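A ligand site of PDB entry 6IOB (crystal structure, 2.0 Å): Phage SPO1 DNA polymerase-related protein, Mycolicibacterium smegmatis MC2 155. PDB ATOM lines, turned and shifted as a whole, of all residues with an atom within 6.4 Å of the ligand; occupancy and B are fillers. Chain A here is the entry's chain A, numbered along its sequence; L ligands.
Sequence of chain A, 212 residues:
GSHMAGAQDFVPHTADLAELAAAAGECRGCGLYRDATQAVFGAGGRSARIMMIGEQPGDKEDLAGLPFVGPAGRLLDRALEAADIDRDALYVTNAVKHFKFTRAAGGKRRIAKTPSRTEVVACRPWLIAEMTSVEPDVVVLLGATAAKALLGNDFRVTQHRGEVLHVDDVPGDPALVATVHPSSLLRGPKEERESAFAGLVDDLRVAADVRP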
ATOM      1  N   GLY A   6     -31.066  17.978   8.448  1.00  0.00           N
ATOM      2  CA  GLY A   6     -29.869  17.664   7.675  1.00  0.00           C
ATOM      3  C   GLY A   6     -29.005  16.633   8.365  1.00  0.00           C
ATOM      4  O   GLY A   6     -29.504  15.613   8.858  1.00  0.00           O
ATOM      5  N   ALA A   7     -27.698  16.890   8.430  1.00  0.00           N
ATOM      6  CA  ALA A   7     -26.741  15.903   8.919  1.00  0.00           C
ATOM      7  C   ALA A   7     -26.794  15.738  10.440  1.00  0.00           C
ATOM      8  O   ALA A   7     -26.093  14.868  10.962  1.00  0.00           O
ATOM      9  CB  ALA A   7     -25.317  16.280   8.517  1.00  0.00           C
ATOM     10  N   PHE A  10     -27.046  12.398  12.002  1.00  0.00           N
ATOM     11  CA  PHE A  10     -25.990  11.455  11.677  1.00  0.00           C
ATOM     12  C   PHE A  10     -24.674  11.723  12.417  1.00  0.00           C
ATOM     13  O   PHE A  10     -23.767  10.888  12.351  1.00  0.00           O
ATOM     14  CB  PHE A  10     -25.779  11.456  10.167  1.00  0.00           C
ATOM     15  CG  PHE A  10     -26.998  10.975   9.422  1.00  0.00           C
ATOM     16  CD1 PHE A  10     -27.303   9.630   9.265  1.00  0.00           C
ATOM     17  CD2 PHE A  10     -27.837  11.918   8.867  1.00  0.00           C
ATOM     18  CE1 PHE A  10     -28.485   9.259   8.589  1.00  0.00           C
ATOM     19  CE2 PHE A  10     -28.974  11.567   8.190  1.00  0.00           C
ATOM     20  CZ  PHE A  10     -29.305  10.242   8.042  1.00  0.00           C
ATOM     21  N   ALA A  24     -19.263   9.961   9.151  1.00  0.00           N
ATOM     22  CA  ALA A  24     -19.677  10.784   8.024  1.00  0.00           C
ATOM     23  C   ALA A  24     -19.878   9.949   6.777  1.00  0.00           C
ATOM     24  O   ALA A  24     -20.765  10.259   5.965  1.00  0.00           O
ATOM     25  CB  ALA A  24     -18.654  11.884   7.759  1.00  0.00           C
ATOM     26  N   CYS A  27     -23.539   9.269   6.523  1.00  0.00           N
ATOM     27  CA  CYS A  27     -24.481  10.373   6.511  1.00  0.00           C
ATOM     28  C   CYS A  27     -25.427  10.309   5.308  1.00  0.00           C
ATOM     29  O   CYS A  27     -24.991  10.069   4.183  1.00  0.00           O
ATOM     30  CB  CYS A  27     -23.700  11.674   6.492  1.00  0.00           C
ATOM     31  SG  CYS A  27     -24.792  13.067   6.767  1.00  0.00           S
ATOM     32  N   ARG A  28     -26.733  10.566   5.526  1.00  0.00           N
ATOM     33  CA  ARG A  28     -27.689  10.803   4.431  1.00  0.00           C
ATOM     34  C   ARG A  28     -28.351  12.173   4.584  1.00  0.00           C
ATOM     35  O   ARG A  28     -29.534  12.329   4.268  1.00  0.00           O
ATOM     36  CB  ARG A  28     -28.732   9.679   4.380  1.00  0.00           C
ATOM     37  CG  ARG A  28     -28.115   8.272   4.394  1.00  0.00           C
ATOM     38  CD  ARG A  28     -29.147   7.127   4.293  1.00  0.00           C
ATOM     39  NE  ARG A  28     -30.175   7.250   5.314  1.00  0.00           N
ATOM     40  CZ  ARG A  28     -30.053   6.686   6.509  1.00  0.00           C
ATOM     41  NH1 ARG A  28     -28.957   5.971   6.779  1.00  0.00           N
ATOM     42  NH2 ARG A  28     -30.976   6.834   7.446  1.00  0.00           N
ATOM     43  N   GLY A  29     -27.582  13.143   5.130  1.00  0.00           N
ATOM     44  CA  GLY A  29     -28.124  14.462   5.428  1.00  0.00           C
ATOM     45  C   GLY A  29     -28.621  15.246   4.242  1.00  0.00           C
ATOM     46  O   GLY A  29     -29.447  16.151   4.399  1.00  0.00           O
ATOM     47  N   CYS A  30     -28.112  14.944   3.076  1.00  0.00           N
ATOM     48  CA  CYS A  30     -28.615  15.548   1.870  1.00  0.00           C
ATOM     49  C   CYS A  30     -28.503  14.478   0.795  1.00  0.00           C
ATOM     50  O   CYS A  30     -28.158  13.333   1.052  1.00  0.00           O
ATOM     51  CB  CYS A  30     -27.857  16.805   1.567  1.00  0.00           C
ATOM     52  SG  CYS A  30     -26.242  16.612   0.872  1.00  0.00           S
ATOM     53  N   GLY A  31     -28.771  14.855  -0.450  1.00  0.00           N
ATOM     54  CA  GLY A  31     -28.738  13.808  -1.451  1.00  0.00           C
ATOM     55  C   GLY A  31     -27.343  13.395  -1.867  1.00  0.00           C
ATOM     56  O   GLY A  31     -27.182  12.409  -2.569  1.00  0.00           O
ATOM     57  N   LEU A  32     -26.322  14.105  -1.473  1.00  0.00           N
ATOM     58  CA  LEU A  32     -25.075  13.872  -2.159  1.00  0.00           C
ATOM     59  C   LEU A  32     -24.395  12.550  -1.799  1.00  0.00           C
ATOM     60  O   LEU A  32     -23.555  12.095  -2.568  1.00  0.00           O
ATOM     61  CB  LEU A  32     -24.191  15.036  -1.785  1.00  0.00           C
ATOM     62  CG  LEU A  32     -24.764  16.353  -2.306  1.00  0.00           C
ATOM     63  CD1 LEU A  32     -23.819  17.474  -1.969  1.00  0.00           C
ATOM     64  CD2 LEU A  32     -24.922  16.273  -3.807  1.00  0.00           C
ATOM     65  N   TYR A  33     -24.789  11.887  -0.707  1.00  0.00           N
ATOM     66  CA  TYR A  33     -24.145  10.615  -0.387  1.00  0.00           C
ATOM     67  C   TYR A  33     -24.462   9.526  -1.393  1.00  0.00           C
ATOM     68  O   TYR A  33     -23.693   8.555  -1.476  1.00  0.00           O
ATOM     69  CB  TYR A  33     -24.594  10.088   0.974  1.00  0.00           C
ATOM     70  CG  TYR A  33     -26.014   9.534   0.976  1.00  0.00           C
ATOM     71  CD1 TYR A  33     -26.239   8.157   0.812  1.00  0.00           C
ATOM     72  CD2 TYR A  33     -27.123  10.364   1.027  1.00  0.00           C
ATOM     73  CE1 TYR A  33     -27.516   7.639   0.768  1.00  0.00           C
ATOM     74  CE2 TYR A  33     -28.409   9.846   0.979  1.00  0.00           C
ATOM     75  CZ  TYR A  33     -28.606   8.479   0.849  1.00  0.00           C
ATOM     76  OH  TYR A  33     -29.874   7.970   0.809  1.00  0.00           O
ATOM     77  N   ALA A  39     -17.573   9.671   1.921  1.00  0.00           N
ATOM     78  CA  ALA A  39     -17.475  11.008   2.479  1.00  0.00           C
ATOM     79  C   ALA A  39     -16.025  11.440   2.407  1.00  0.00           C
ATOM     80  O   ALA A  39     -15.117  10.629   2.604  1.00  0.00           O
ATOM     81  CB  ALA A  39     -17.955  11.014   3.932  1.00  0.00           C
ATOM     82  N   ALA A  95     -16.706  22.616   3.236  1.00  0.00           N
ATOM     83  CA  ALA A  95     -18.048  22.879   3.724  1.00  0.00           C
ATOM     84  C   ALA A  95     -18.978  21.698   3.473  1.00  0.00           C
ATOM     85  O   ALA A  95     -19.886  21.444   4.263  1.00  0.00           O
ATOM     86  CB  ALA A  95     -18.617  24.154   3.097  1.00  0.00           C
ATOM     87  N   VAL A  96     -18.814  21.045   2.323  1.00  0.00           N
ATOM     88  CA  VAL A  96     -19.649  19.920   1.915  1.00  0.00           C
ATOM     89  C   VAL A  96     -18.746  18.703   1.747  1.00  0.00           C
ATOM     90  O   VAL A  96     -17.681  18.796   1.133  1.00  0.00           O
ATOM     91  CB  VAL A  96     -20.381  20.268   0.601  1.00  0.00           C
ATOM     92  CG1 VAL A  96     -20.950  19.051  -0.078  1.00  0.00           C
ATOM     93  CG2 VAL A  96     -21.468  21.321   0.876  1.00  0.00           C
ATOM     94  N   LYS A  97     -19.156  17.562   2.306  1.00  0.00           N
ATOM     95  CA  LYS A  97     -18.284  16.401   2.398  1.00  0.00           C
ATOM     96  C   LYS A  97     -18.509  15.299   1.357  1.00  0.00           C
ATOM     97  O   LYS A  97     -17.803  14.301   1.411  1.00  0.00           O
ATOM     98  CB  LYS A  97     -18.279  15.873   3.824  1.00  0.00           C
ATOM     99  CG  LYS A  97     -17.821  17.026   4.696  1.00  0.00           C
ATOM    100  CD  LYS A  97     -17.780  16.778   6.175  1.00  0.00           C
ATOM    101  CE  LYS A  97     -16.688  17.660   6.805  1.00  0.00           C
ATOM    102  NZ  LYS A  97     -16.990  19.119   6.802  1.00  0.00           N
ATOM    103  N   HIS A  98     -19.532  15.372   0.521  1.00  0.00           N
ATOM    104  CA  HIS A  98     -19.723  14.429  -0.586  1.00  0.00           C
ATOM    105  C   HIS A  98     -19.642  15.106  -1.932  1.00  0.00           C
ATOM    106  O   HIS A  98     -20.056  16.234  -2.110  1.00  0.00           O
ATOM    107  CB  HIS A  98     -20.995  13.623  -0.509  1.00  0.00           C
ATOM    108  CG  HIS A  98     -20.920  12.536   0.480  1.00  0.00           C
ATOM    109  ND1 HIS A  98     -21.498  12.691   1.696  1.00  0.00           N
ATOM    110  CD2 HIS A  98     -20.293  11.320   0.505  1.00  0.00           C
ATOM    111  CE1 HIS A  98     -21.342  11.608   2.415  1.00  0.00           C
ATOM    112  NE2 HIS A  98     -20.595  10.747   1.714  1.00  0.00           N
ATOM    113  N   GLU A 119     -27.757  22.167   0.462  1.00  0.00           N
ATOM    114  CA  GLU A 119     -26.784  21.137   0.795  1.00  0.00           C
ATOM    115  C   GLU A 119     -25.748  21.686   1.772  1.00  0.00           C
ATOM    116  O   GLU A 119     -25.329  20.989   2.700  1.00  0.00           O
ATOM    117  CB  GLU A 119     -26.141  20.599  -0.481  1.00  0.00           C
ATOM    118  CG  GLU A 119     -27.055  19.739  -1.328  1.00  0.00           C
ATOM    119  CD  GLU A 119     -26.759  19.758  -2.810  1.00  0.00           C
ATOM    120  OE1 GLU A 119     -25.990  20.631  -3.274  1.00  0.00           O
ATOM    121  OE2 GLU A 119     -27.248  18.849  -3.505  1.00  0.00           O
ATOM    122  N   ALA A 122     -27.243  21.667   5.071  1.00  0.00           N
ATOM    123  CA  ALA A 122     -27.390  20.287   5.526  1.00  0.00           C
ATOM    124  C   ALA A 122     -26.085  19.722   6.065  1.00  0.00           C
ATOM    125  O   ALA A 122     -26.082  18.957   7.034  1.00  0.00           O
ATOM    126  CB  ALA A 122     -27.938  19.413   4.407  1.00  0.00           C
ATOM    127  N   CYS A 123     -24.974  20.114   5.485  1.00  0.00           N
ATOM    128  CA  CYS A 123     -23.724  19.508   5.878  1.00  0.00           C
ATOM    129  C   CYS A 123     -23.046  20.259   6.994  1.00  0.00           C
ATOM    130  O   CYS A 123     -22.100  19.724   7.598  1.00  0.00           O
ATOM    131  CB  CYS A 123     -22.805  19.385   4.663  1.00  0.00           C
ATOM    132  SG  CYS A 123     -21.515  18.132   4.729  1.00  0.00           S
ATOM    133  N   ARG A 124     -23.471  21.494   7.227  1.00  0.00           N
ATOM    134  CA  ARG A 124     -22.860  22.365   8.232  1.00  0.00           C
ATOM    135  C   ARG A 124     -22.688  21.732   9.650  1.00  0.00           C
ATOM    136  O   ARG A 124     -21.686  22.038  10.332  1.00  0.00           O
ATOM    137  CB  ARG A 124     -23.700  23.639   8.361  1.00  0.00           C
ATOM    138  CG  ARG A 124     -22.941  24.662   9.121  1.00  0.00           C
ATOM    139  CD  ARG A 124     -23.710  25.899   9.526  1.00  0.00           C
ATOM    140  NE  ARG A 124     -24.822  26.337   8.849  1.00  0.00           N
ATOM    141  CZ  ARG A 124     -25.394  27.376   9.108  1.00  0.00           C
ATOM    142  NH1 ARG A 124     -26.413  27.732   8.465  1.00  0.00           N
ATOM    143  NH2 ARG A 124     -24.948  28.040  10.032  1.00  0.00           N
ATOM    144  N   TRP A 126     -21.514  18.923  10.432  1.00  0.00           N
ATOM    145  CA  TRP A 126     -20.196  18.299  10.438  1.00  0.00           C
ATOM    146  C   TRP A 126     -19.111  19.345  10.633  1.00  0.00           C
ATOM    147  O   TRP A 126     -18.119  19.100  11.315  1.00  0.00           O
ATOM    148  CB  TRP A 126     -19.941  17.512   9.157  1.00  0.00           C
ATOM    149  CG  TRP A 126     -20.784  16.290   9.002  1.00  0.00           C
ATOM    150  CD1 TRP A 126     -21.769  16.061   8.094  1.00  0.00           C
ATOM    151  CD2 TRP A 126     -20.691  15.110   9.805  1.00  0.00           C
ATOM    152  NE1 TRP A 126     -22.297  14.807   8.283  1.00  0.00           N
ATOM    153  CE2 TRP A 126     -21.652  14.197   9.322  1.00  0.00           C
ATOM    154  CE3 TRP A 126     -19.882  14.736  10.880  1.00  0.00           C
ATOM    155  CZ2 TRP A 126     -21.828  12.940   9.893  1.00  0.00           C
ATOM    156  CZ3 TRP A 126     -20.067  13.480  11.446  1.00  0.00           C
ATOM    157  CH2 TRP A 126     -21.029  12.596  10.941  1.00  0.00           C
HETATM  158 FE1  LIG L   1     -22.760  16.413   4.062  1.00  0.00          FE
HETATM  159 FE2  LIG L   1     -24.359  14.247   4.940  1.00  0.00          FE
HETATM  160 FE3  LIG L   1     -22.832  13.901   2.635  1.00  0.00          FE
HETATM  161 FE4  LIG L   1     -25.083  15.647   2.477  1.00  0.00          FE
HETATM  162  S1  LIG L   1     -24.966  13.531   2.975  1.00  0.00           S
HETATM  163  S2  LIG L   1     -23.011  15.935   1.957  1.00  0.00           S
HETATM  164  S3  LIG L   1     -24.877  16.315   4.546  1.00  0.00           S
HETATM  165  S4  LIG L   1     -22.206  14.397   4.692  1.00  0.00           S
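The side-chain sulfur (SG) of Cys 27 is bound to an iron atom (FE2) of the ligand. S1 of the ligand lies close to N of Cys 30 (3.5 Å). FE1 of the ligand is bound by SG of Cys 123 (2.2 Å). N of Gly 29 lies close to S1 of the ligand, at 3.4 Å. The side-chain sulfur (SG) of Cys 30 binds an iron atom (FE4) of the ligand, 2.2 Å away. A sulfur (S4) of the ligand lies close to the indole nitrogen of Trp 126, 3.6 Å away. An iron atom (FE3) of the ligand is bound by a ring nitrogen (ND1) of His 98 (2.0 Å).
NE2 of His 98 lies within hydrogen-bond range of N of Ala 39. The backbone carbonyl oxygen of Ala 122 sits at hydrogen-bond distance from the backbone NH of Ala 7, at 3.0 Å. The side-chain sulfur (SG) of Cys 123 sits close to the backbone carbonyl oxygen (O) of Ala 95 (3.7 Å). The side-chain sulfur of Cys 27 lies close to the backbone NH of Gly 29 (3.2 Å). SG of Cys 123 lies close to N of Lys 97 (3.4 Å). SG of Cys 27 sits close to NE1 of Trp 126, 3.4 Å away. SG of Cys 30 sits close to N of Leu 32, at 3.4 Å.
Residues that only touch the ligand: Ala 122, Arg 28, Ala 7 and Tyr 33. Hydrophobic or aromatic side chains within 4 Å of the ligand: Ala 7, Tyr 33, His 98 and Trp 126. Ten residues have an atom within 4 Å of the ligand: Ala 7, Cys 27, Arg 28, Gly 29, Cys 30, Tyr 33, His 98, Ala 122, Cys 123 and Trp 126.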
